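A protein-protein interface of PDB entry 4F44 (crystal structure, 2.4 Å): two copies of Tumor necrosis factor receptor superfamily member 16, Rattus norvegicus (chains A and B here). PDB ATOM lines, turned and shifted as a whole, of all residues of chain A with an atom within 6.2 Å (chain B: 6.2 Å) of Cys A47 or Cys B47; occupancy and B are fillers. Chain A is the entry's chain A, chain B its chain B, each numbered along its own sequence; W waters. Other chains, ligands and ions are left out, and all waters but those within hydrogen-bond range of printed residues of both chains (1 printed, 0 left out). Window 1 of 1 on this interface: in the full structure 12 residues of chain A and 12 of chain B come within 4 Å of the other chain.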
ATOM      1  N   GLU A  17     -11.498 -17.786   9.862  1.00  0.00           N
ATOM      2  CA  GLU A  17     -10.950 -16.948  10.922  1.00  0.00           C
ATOM      3  C   GLU A  17     -11.657 -17.123  12.265  1.00  0.00           C
ATOM      4  O   GLU A  17     -10.996 -17.170  13.313  1.00  0.00           O
ATOM      5  CB  GLU A  17     -10.958 -15.490  10.503  1.00  0.00           C
ATOM      6  CG  GLU A  17     -10.051 -15.167   9.348  1.00  0.00           C
ATOM      7  CD  GLU A  17     -10.384 -13.812   8.764  1.00  0.00           C
ATOM      8  OE1 GLU A  17     -11.219 -13.114   9.377  1.00  0.00           O
ATOM      9  OE2 GLU A  17      -9.835 -13.443   7.703  1.00  0.00           O
ATOM     10  N   PHE A  42       2.929 -10.645  14.176  1.00  0.00           N
ATOM     11  CA  PHE A  42       1.542 -10.490  13.699  1.00  0.00           C
ATOM     12  C   PHE A  42       0.544 -10.020  14.778  1.00  0.00           C
ATOM     13  O   PHE A  42      -0.508  -9.461  14.453  1.00  0.00           O
ATOM     14  CB  PHE A  42       1.048 -11.750  12.983  1.00  0.00           C
ATOM     15  CG  PHE A  42       1.617 -11.925  11.592  1.00  0.00           C
ATOM     16  CD1 PHE A  42       1.138 -11.160  10.530  1.00  0.00           C
ATOM     17  CD2 PHE A  42       2.640 -12.843  11.351  1.00  0.00           C
ATOM     18  CE1 PHE A  42       1.650 -11.328   9.250  1.00  0.00           C
ATOM     19  CE2 PHE A  42       3.170 -13.017  10.070  1.00  0.00           C
ATOM     20  CZ  PHE A  42       2.688 -12.255   9.014  1.00  0.00           C
ATOM     21  N   HIS A  44       0.735  -7.476  16.287  1.00  0.00           N
ATOM     22  CA  HIS A  44       0.723  -6.013  16.237  1.00  0.00           C
ATOM     23  C   HIS A  44      -0.389  -5.533  15.348  1.00  0.00           C
ATOM     24  O   HIS A  44      -0.737  -4.350  15.345  1.00  0.00           O
ATOM     25  CB  HIS A  44       2.068  -5.448  15.772  1.00  0.00           C
ATOM     26  CG  HIS A  44       3.125  -5.526  16.824  1.00  0.00           C
ATOM     27  ND1 HIS A  44       3.974  -6.607  16.949  1.00  0.00           N
ATOM     28  CD2 HIS A  44       3.411  -4.699  17.857  1.00  0.00           C
ATOM     29  CE1 HIS A  44       4.756  -6.425  17.999  1.00  0.00           C
ATOM     30  NE2 HIS A  44       4.435  -5.274  18.564  1.00  0.00           N
ATOM     31  N   GLU A  45      -0.953  -6.470  14.599  1.00  0.00           N
ATOM     32  CA  GLU A  45      -1.992  -6.174  13.644  1.00  0.00           C
ATOM     33  C   GLU A  45      -3.308  -6.080  14.398  1.00  0.00           C
ATOM     34  O   GLU A  45      -3.432  -6.607  15.504  1.00  0.00           O
ATOM     35  CB  GLU A  45      -2.055  -7.297  12.602  1.00  0.00           C
ATOM     36  CG  GLU A  45      -0.757  -7.531  11.823  1.00  0.00           C
ATOM     37  CD  GLU A  45      -0.353  -6.337  10.994  1.00  0.00           C
ATOM     38  OE1 GLU A  45      -1.241  -5.513  10.663  1.00  0.00           O
ATOM     39  OE2 GLU A  45       0.862  -6.200  10.713  1.00  0.00           O
ATOM     40  N   ALA A  46      -4.278  -5.389  13.808  1.00  0.00           N
ATOM     41  CA  ALA A  46      -5.604  -5.262  14.401  1.00  0.00           C
ATOM     42  C   ALA A  46      -6.306  -6.621  14.386  1.00  0.00           C
ATOM     43  O   ALA A  46      -7.177  -6.879  15.216  1.00  0.00           O
ATOM     44  CB  ALA A  46      -6.424  -4.244  13.636  1.00  0.00           C
ATOM     45  N   CYS A  47      -5.910  -7.466  13.438  1.00  0.00           N
ATOM     46  CA  CYS A  47      -6.537  -8.756  13.207  1.00  0.00           C
ATOM     47  C   CYS A  47      -5.473  -9.789  12.836  1.00  0.00           C
ATOM     48  O   CYS A  47      -5.335 -10.156  11.664  1.00  0.00           O
ATOM     49  CB  CYS A  47      -7.567  -8.623  12.087  1.00  0.00           C
ATOM     50  SG  CYS A  47      -8.644 -10.057  11.948  1.00  0.00           S
ATOM     51  N   PRO A  48      -4.675 -10.221  13.828  1.00  0.00           N
ATOM     52  CA  PRO A  48      -3.531 -11.087  13.571  1.00  0.00           C
ATOM     53  C   PRO A  48      -3.852 -12.265  12.656  1.00  0.00           C
ATOM     54  O   PRO A  48      -3.073 -12.568  11.749  1.00  0.00           O
ATOM     55  CB  PRO A  48      -3.146 -11.583  14.987  1.00  0.00           C
ATOM     56  CG  PRO A  48      -3.586 -10.486  15.893  1.00  0.00           C
ATOM     57  CD  PRO A  48      -4.862  -9.968  15.274  1.00  0.00           C
ATOM     58  N   VAL A  49      -4.988 -12.925  12.872  1.00  0.00           N
ATOM     59  CA  VAL A  49      -5.310 -14.119  12.099  1.00  0.00           C
ATOM     60  C   VAL A  49      -5.503 -13.807  10.609  1.00  0.00           C
ATOM     61  O   VAL A  49      -5.025 -14.554   9.749  1.00  0.00           O
ATOM     62  CB  VAL A  49      -6.500 -14.921  12.689  1.00  0.00           C
ATOM     63  CG1 VAL A  49      -7.843 -14.120  12.639  1.00  0.00           C
ATOM     64  CG2 VAL A  49      -6.655 -16.274  11.974  1.00  0.00           C
ATOM     65  N   ARG A  50      -6.143 -12.687  10.292  1.00  0.00           N
ATOM     66  CA  ARG A  50      -6.344 -12.313   8.893  1.00  0.00           C
ATOM     67  C   ARG A  50      -5.016 -11.959   8.242  1.00  0.00           C
ATOM     68  O   ARG A  50      -4.722 -12.391   7.134  1.00  0.00           O
ATOM     69  CB  ARG A  50      -7.309 -11.137   8.775  1.00  0.00           C
ATOM     70  CG  ARG A  50      -7.665 -10.743   7.321  1.00  0.00           C
ATOM     71  CD  ARG A  50      -8.594  -9.516   7.273  1.00  0.00           C
ATOM     72  NE  ARG A  50      -9.834  -9.757   7.992  1.00  0.00           N
ATOM     73  CZ  ARG A  50     -10.425  -8.893   8.825  1.00  0.00           C
ATOM     74  NH1 ARG A  50      -9.904  -7.682   9.079  1.00  0.00           N
ATOM     75  NH2 ARG A  50     -11.559  -9.252   9.423  1.00  0.00           N
ATOM     76  N   ALA A  51      -4.200 -11.199   8.963  1.00  0.00           N
ATOM     77  CA  ALA A  51      -2.935 -10.698   8.436  1.00  0.00           C
ATOM     78  C   ALA A  51      -1.996 -11.860   8.182  1.00  0.00           C
ATOM     79  O   ALA A  51      -1.374 -11.928   7.127  1.00  0.00           O
ATOM     80  CB  ALA A  51      -2.308  -9.705   9.414  1.00  0.00           C
ATOM     81  N   LEU A  52      -1.880 -12.772   9.148  1.00  0.00           N
ATOM     82  CA  LEU A  52      -1.108 -13.993   8.912  1.00  0.00           C
ATOM     83  C   LEU A  52      -1.573 -14.689   7.625  1.00  0.00           C
ATOM     84  O   LEU A  52      -0.772 -14.976   6.739  1.00  0.00           O
ATOM     85  CB  LEU A  52      -1.185 -14.960  10.103  1.00  0.00           C
ATOM     86  CG  LEU A  52      -0.437 -16.242   9.705  1.00  0.00           C
ATOM     87  CD1 LEU A  52       1.033 -16.207  10.128  1.00  0.00           C
ATOM     88  CD2 LEU A  52      -1.140 -17.527  10.177  1.00  0.00           C
ATOM     89  N   GLU B  17     -12.446  -2.420   9.649  1.00  0.00           N
ATOM     90  CA  GLU B  17     -11.401  -3.140  10.373  1.00  0.00           C
ATOM     91  C   GLU B  17      -9.997  -2.893   9.823  1.00  0.00           C
ATOM     92  O   GLU B  17      -9.053  -2.689  10.586  1.00  0.00           O
ATOM     93  CB  GLU B  17     -11.706  -4.630  10.390  1.00  0.00           C
ATOM     94  CG  GLU B  17     -12.936  -5.003  11.184  1.00  0.00           C
ATOM     95  CD  GLU B  17     -13.422  -6.404  10.859  1.00  0.00           C
ATOM     96  OE1 GLU B  17     -12.693  -7.133  10.157  1.00  0.00           O
ATOM     97  OE2 GLU B  17     -14.529  -6.777  11.292  1.00  0.00           O
ATOM     98  N   PHE B  42      -9.530  -8.190  24.851  1.00  0.00           N
ATOM     99  CA  PHE B  42      -9.747  -8.495  23.435  1.00  0.00           C
ATOM    100  C   PHE B  42      -8.478  -8.922  22.660  1.00  0.00           C
ATOM    101  O   PHE B  42      -8.589  -9.614  21.641  1.00  0.00           O
ATOM    102  CB  PHE B  42     -10.499  -7.362  22.723  1.00  0.00           C
ATOM    103  CG  PHE B  42     -11.930  -7.186  23.188  1.00  0.00           C
ATOM    104  CD1 PHE B  42     -12.927  -8.030  22.728  1.00  0.00           C
ATOM    105  CD2 PHE B  42     -12.273  -6.177  24.095  1.00  0.00           C
ATOM    106  CE1 PHE B  42     -14.254  -7.861  23.154  1.00  0.00           C
ATOM    107  CE2 PHE B  42     -13.595  -6.022  24.543  1.00  0.00           C
ATOM    108  CZ  PHE B  42     -14.587  -6.857  24.070  1.00  0.00           C
ATOM    109  N   HIS B  44      -6.816 -11.271  23.385  1.00  0.00           N
ATOM    110  CA  HIS B  44      -6.778 -12.730  23.437  1.00  0.00           C
ATOM    111  C   HIS B  44      -7.469 -13.344  22.248  1.00  0.00           C
ATOM    112  O   HIS B  44      -7.251 -14.513  21.936  1.00  0.00           O
ATOM    113  CB  HIS B  44      -7.345 -13.274  24.750  1.00  0.00           C
ATOM    114  CG  HIS B  44      -6.537 -12.874  25.945  1.00  0.00           C
ATOM    115  ND1 HIS B  44      -5.497 -13.640  26.430  1.00  0.00           N
ATOM    116  CD2 HIS B  44      -6.571 -11.755  26.710  1.00  0.00           C
ATOM    117  CE1 HIS B  44      -4.940 -13.025  27.456  1.00  0.00           C
ATOM    118  NE2 HIS B  44      -5.571 -11.877  27.646  1.00  0.00           N
ATOM    119  N   GLU B  45      -8.289 -12.551  21.567  1.00  0.00           N
ATOM    120  CA  GLU B  45      -9.056 -13.044  20.433  1.00  0.00           C
ATOM    121  C   GLU B  45      -8.142 -13.093  19.223  1.00  0.00           C
ATOM    122  O   GLU B  45      -7.111 -12.441  19.197  1.00  0.00           O
ATOM    123  CB  GLU B  45     -10.270 -12.142  20.158  1.00  0.00           C
ATOM    124  CG  GLU B  45     -11.340 -12.056  21.277  1.00  0.00           C
ATOM    125  CD  GLU B  45     -11.851 -13.405  21.752  1.00  0.00           C
ATOM    126  OE1 GLU B  45     -11.796 -14.392  20.982  1.00  0.00           O
ATOM    127  OE2 GLU B  45     -12.304 -13.479  22.917  1.00  0.00           O
ATOM    128  N   ALA B  46      -8.507 -13.887  18.227  1.00  0.00           N
ATOM    129  CA  ALA B  46      -7.675 -14.022  17.036  1.00  0.00           C
ATOM    130  C   ALA B  46      -7.744 -12.746  16.185  1.00  0.00           C
ATOM    131  O   ALA B  46      -6.846 -12.484  15.374  1.00  0.00           O
ATOM    132  CB  ALA B  46      -8.103 -15.235  16.222  1.00  0.00           C
ATOM    133  N   CYS B  47      -8.819 -11.983  16.379  1.00  0.00           N
ATOM    134  CA  CYS B  47      -9.072 -10.772  15.610  1.00  0.00           C
ATOM    135  C   CYS B  47      -9.661  -9.722  16.534  1.00  0.00           C
ATOM    136  O   CYS B  47     -10.869  -9.493  16.514  1.00  0.00           O
ATOM    137  CB  CYS B  47     -10.041 -11.071  14.462  1.00  0.00           C
ATOM    138  SG  CYS B  47     -10.163  -9.717  13.234  1.00  0.00           S
ATOM    139  N   PRO B  48      -8.820  -9.134  17.408  1.00  0.00           N
ATOM    140  CA  PRO B  48      -9.312  -8.257  18.452  1.00  0.00           C
ATOM    141  C   PRO B  48     -10.262  -7.193  17.928  1.00  0.00           C
ATOM    142  O   PRO B  48     -11.270  -6.881  18.585  1.00  0.00           O
ATOM    143  CB  PRO B  48      -8.017  -7.600  18.992  1.00  0.00           C
ATOM    144  CG  PRO B  48      -6.979  -8.624  18.795  1.00  0.00           C
ATOM    145  CD  PRO B  48      -7.348  -9.250  17.448  1.00  0.00           C
ATOM    146  N   VAL B  49      -9.963  -6.623  16.764  1.00  0.00           N
ATOM    147  CA  VAL B  49     -10.737  -5.477  16.314  1.00  0.00           C
ATOM    148  C   VAL B  49     -12.174  -5.897  15.988  1.00  0.00           C
ATOM    149  O   VAL B  49     -13.136  -5.214  16.375  1.00  0.00           O
ATOM    150  CB  VAL B  49     -10.067  -4.703  15.149  1.00  0.00           C
ATOM    151  CG1 VAL B  49      -9.882  -5.584  13.890  1.00  0.00           C
ATOM    152  CG2 VAL B  49     -10.884  -3.453  14.811  1.00  0.00           C
ATOM    153  N   ARG B  50     -12.315  -7.044  15.328  1.00  0.00           N
ATOM    154  CA  ARG B  50     -13.636  -7.546  14.974  1.00  0.00           C
ATOM    155  C   ARG B  50     -14.420  -7.894  16.241  1.00  0.00           C
ATOM    156  O   ARG B  50     -15.580  -7.515  16.395  1.00  0.00           O
ATOM    157  CB  ARG B  50     -13.535  -8.764  14.060  1.00  0.00           C
ATOM    158  CG  ARG B  50     -14.902  -9.300  13.583  1.00  0.00           C
ATOM    159  CD  ARG B  50     -14.796 -10.626  12.834  1.00  0.00           C
ATOM    160  NE  ARG B  50     -14.045 -10.511  11.586  1.00  0.00           N
ATOM    161  CZ  ARG B  50     -12.997 -11.275  11.259  1.00  0.00           C
ATOM    162  NH1 ARG B  50     -12.472 -12.124  12.144  1.00  0.00           N
ATOM    163  NH2 ARG B  50     -12.473 -11.195  10.035  1.00  0.00           N
ATOM    164  N   ALA B  51     -13.751  -8.555  17.178  1.00  0.00           N
ATOM    165  CA  ALA B  51     -14.416  -9.027  18.392  1.00  0.00           C
ATOM    166  C   ALA B  51     -14.854  -7.838  19.242  1.00  0.00           C
ATOM    167  O   ALA B  51     -15.978  -7.807  19.731  1.00  0.00           O
ATOM    168  CB  ALA B  51     -13.491  -9.983  19.177  1.00  0.00           C
ATOM    169  N   LEU B  52     -13.996  -6.832  19.382  1.00  0.00           N
ATOM    170  CA  LEU B  52     -14.422  -5.590  20.038  1.00  0.00           C
ATOM    171  C   LEU B  52     -15.667  -4.980  19.393  1.00  0.00           C
ATOM    172  O   LEU B  52     -16.639  -4.653  20.080  1.00  0.00           O
ATOM    173  CB  LEU B  52     -13.286  -4.553  20.100  1.00  0.00           C
ATOM    174  CG  LEU B  52     -13.799  -3.313  20.854  1.00  0.00           C
ATOM    175  CD1 LEU B  52     -13.092  -3.079  22.188  1.00  0.00           C
ATOM    176  CD2 LEU B  52     -13.844  -2.045  19.953  1.00  0.00           C
HETATM  177  O   HOH W   1     -12.666 -11.683   7.025  1.00  0.00           O
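The side-chain carboxylate (OE2) of Glu A17 lies within salt-bridge range of the guanidinium group (NE) of Arg A50, at 3.7 Å.
The guanidinium group of Arg B50 lies within salt-bridge range of the side-chain carboxylate of Glu B17 (3.8 Å).
NH1 of Arg B50 lies within hydrogen-bond range of SG of Cys B47.
Water W1 lies within hydrogen-bond range of the guanidinium group of Arg B50 and the side-chain carboxylate of Glu A17.
Among the printed residues, pairs that only touch across the chains: Ala A46 with Cys B47, Ala A46 with Pro B48, Cys A47 with Ala B46 and Pro A48 with Pro B48.
The side-chain carboxylate (OE1) of Glu A17 is in salt-bridge range of the guanidinium group (NH1) of Arg B50.
O of Ala A46 is in hydrogen-bond range of N of Val B49 (3.2 Å).
The side-chain sulfur of Cys A47 is disulfide-bonded to the side-chain sulfur of Cys B47, at 2.0 Å.
O of Ala B46 sits at hydrogen-bond distance from N of Val A49 (3.1 Å).
The guanidinium group of Arg A50 is in salt-bridge range of the side-chain carboxylate of Glu B17 (2.5 Å).
The backbone carbonyl oxygen (O) of Ala B46 lies close to the backbone nitrogen (N) of Pro A48 (3.5 Å).
NH2 of Arg B50 lies close to NH2 of Arg A50 (2.2 Å).
Of chain B, only Ala B46 and Cys B47 come within 4 Å of Cys A47.
Printed residues of chain A within 4 Å of Cys B47: Ala A46 (3.999 Å) and Cys A47 (2.0 Å).
Of the printed residues of chain A, Pro B48 touches Ala A46 and Pro A48.
Printed residues of chain A within 4 Å of Val B49: Ala A46.
Printed residues of chain A within 4 Å of Arg B50: Glu A17 and Arg A50.
Printed residues of chain B within 4 Å of Ala A46: Cys B47 (3.999 Å), Pro B48 (3.3 Å) and Val B49 (3.2 Å).
The nearest residue of chain B that does not touch Cys A47 is Val B49 (4.2 Å).
Glu A17 touches Arg B50, and with the chains exchanged Arg A50 touches Glu B17.
Ala A46 touches Pro B48, and with the chains exchanged Pro A48 touches Ala B46.
Cys B47 touches its own counterpart, Cys A47.
Pro B48 touches its own counterpart, Pro A48.
11 positions are printed for both chains.
Of the 11 printed residues of chain A, 6 touch a printed residue of chain B.
Hydrophobic or aromatic side chains of chain A within 4 Å of the printed part of chain B: Ala A46, Pro A48 and Val A49.
Among the printed residues, Asp or Glu carboxylates within 4 Å of a Lys or Arg side-chain nitrogen of the other chain: Glu A17 with Arg B50 (2.4 Å) and Arg A50 with Glu B17 (2.5 Å).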
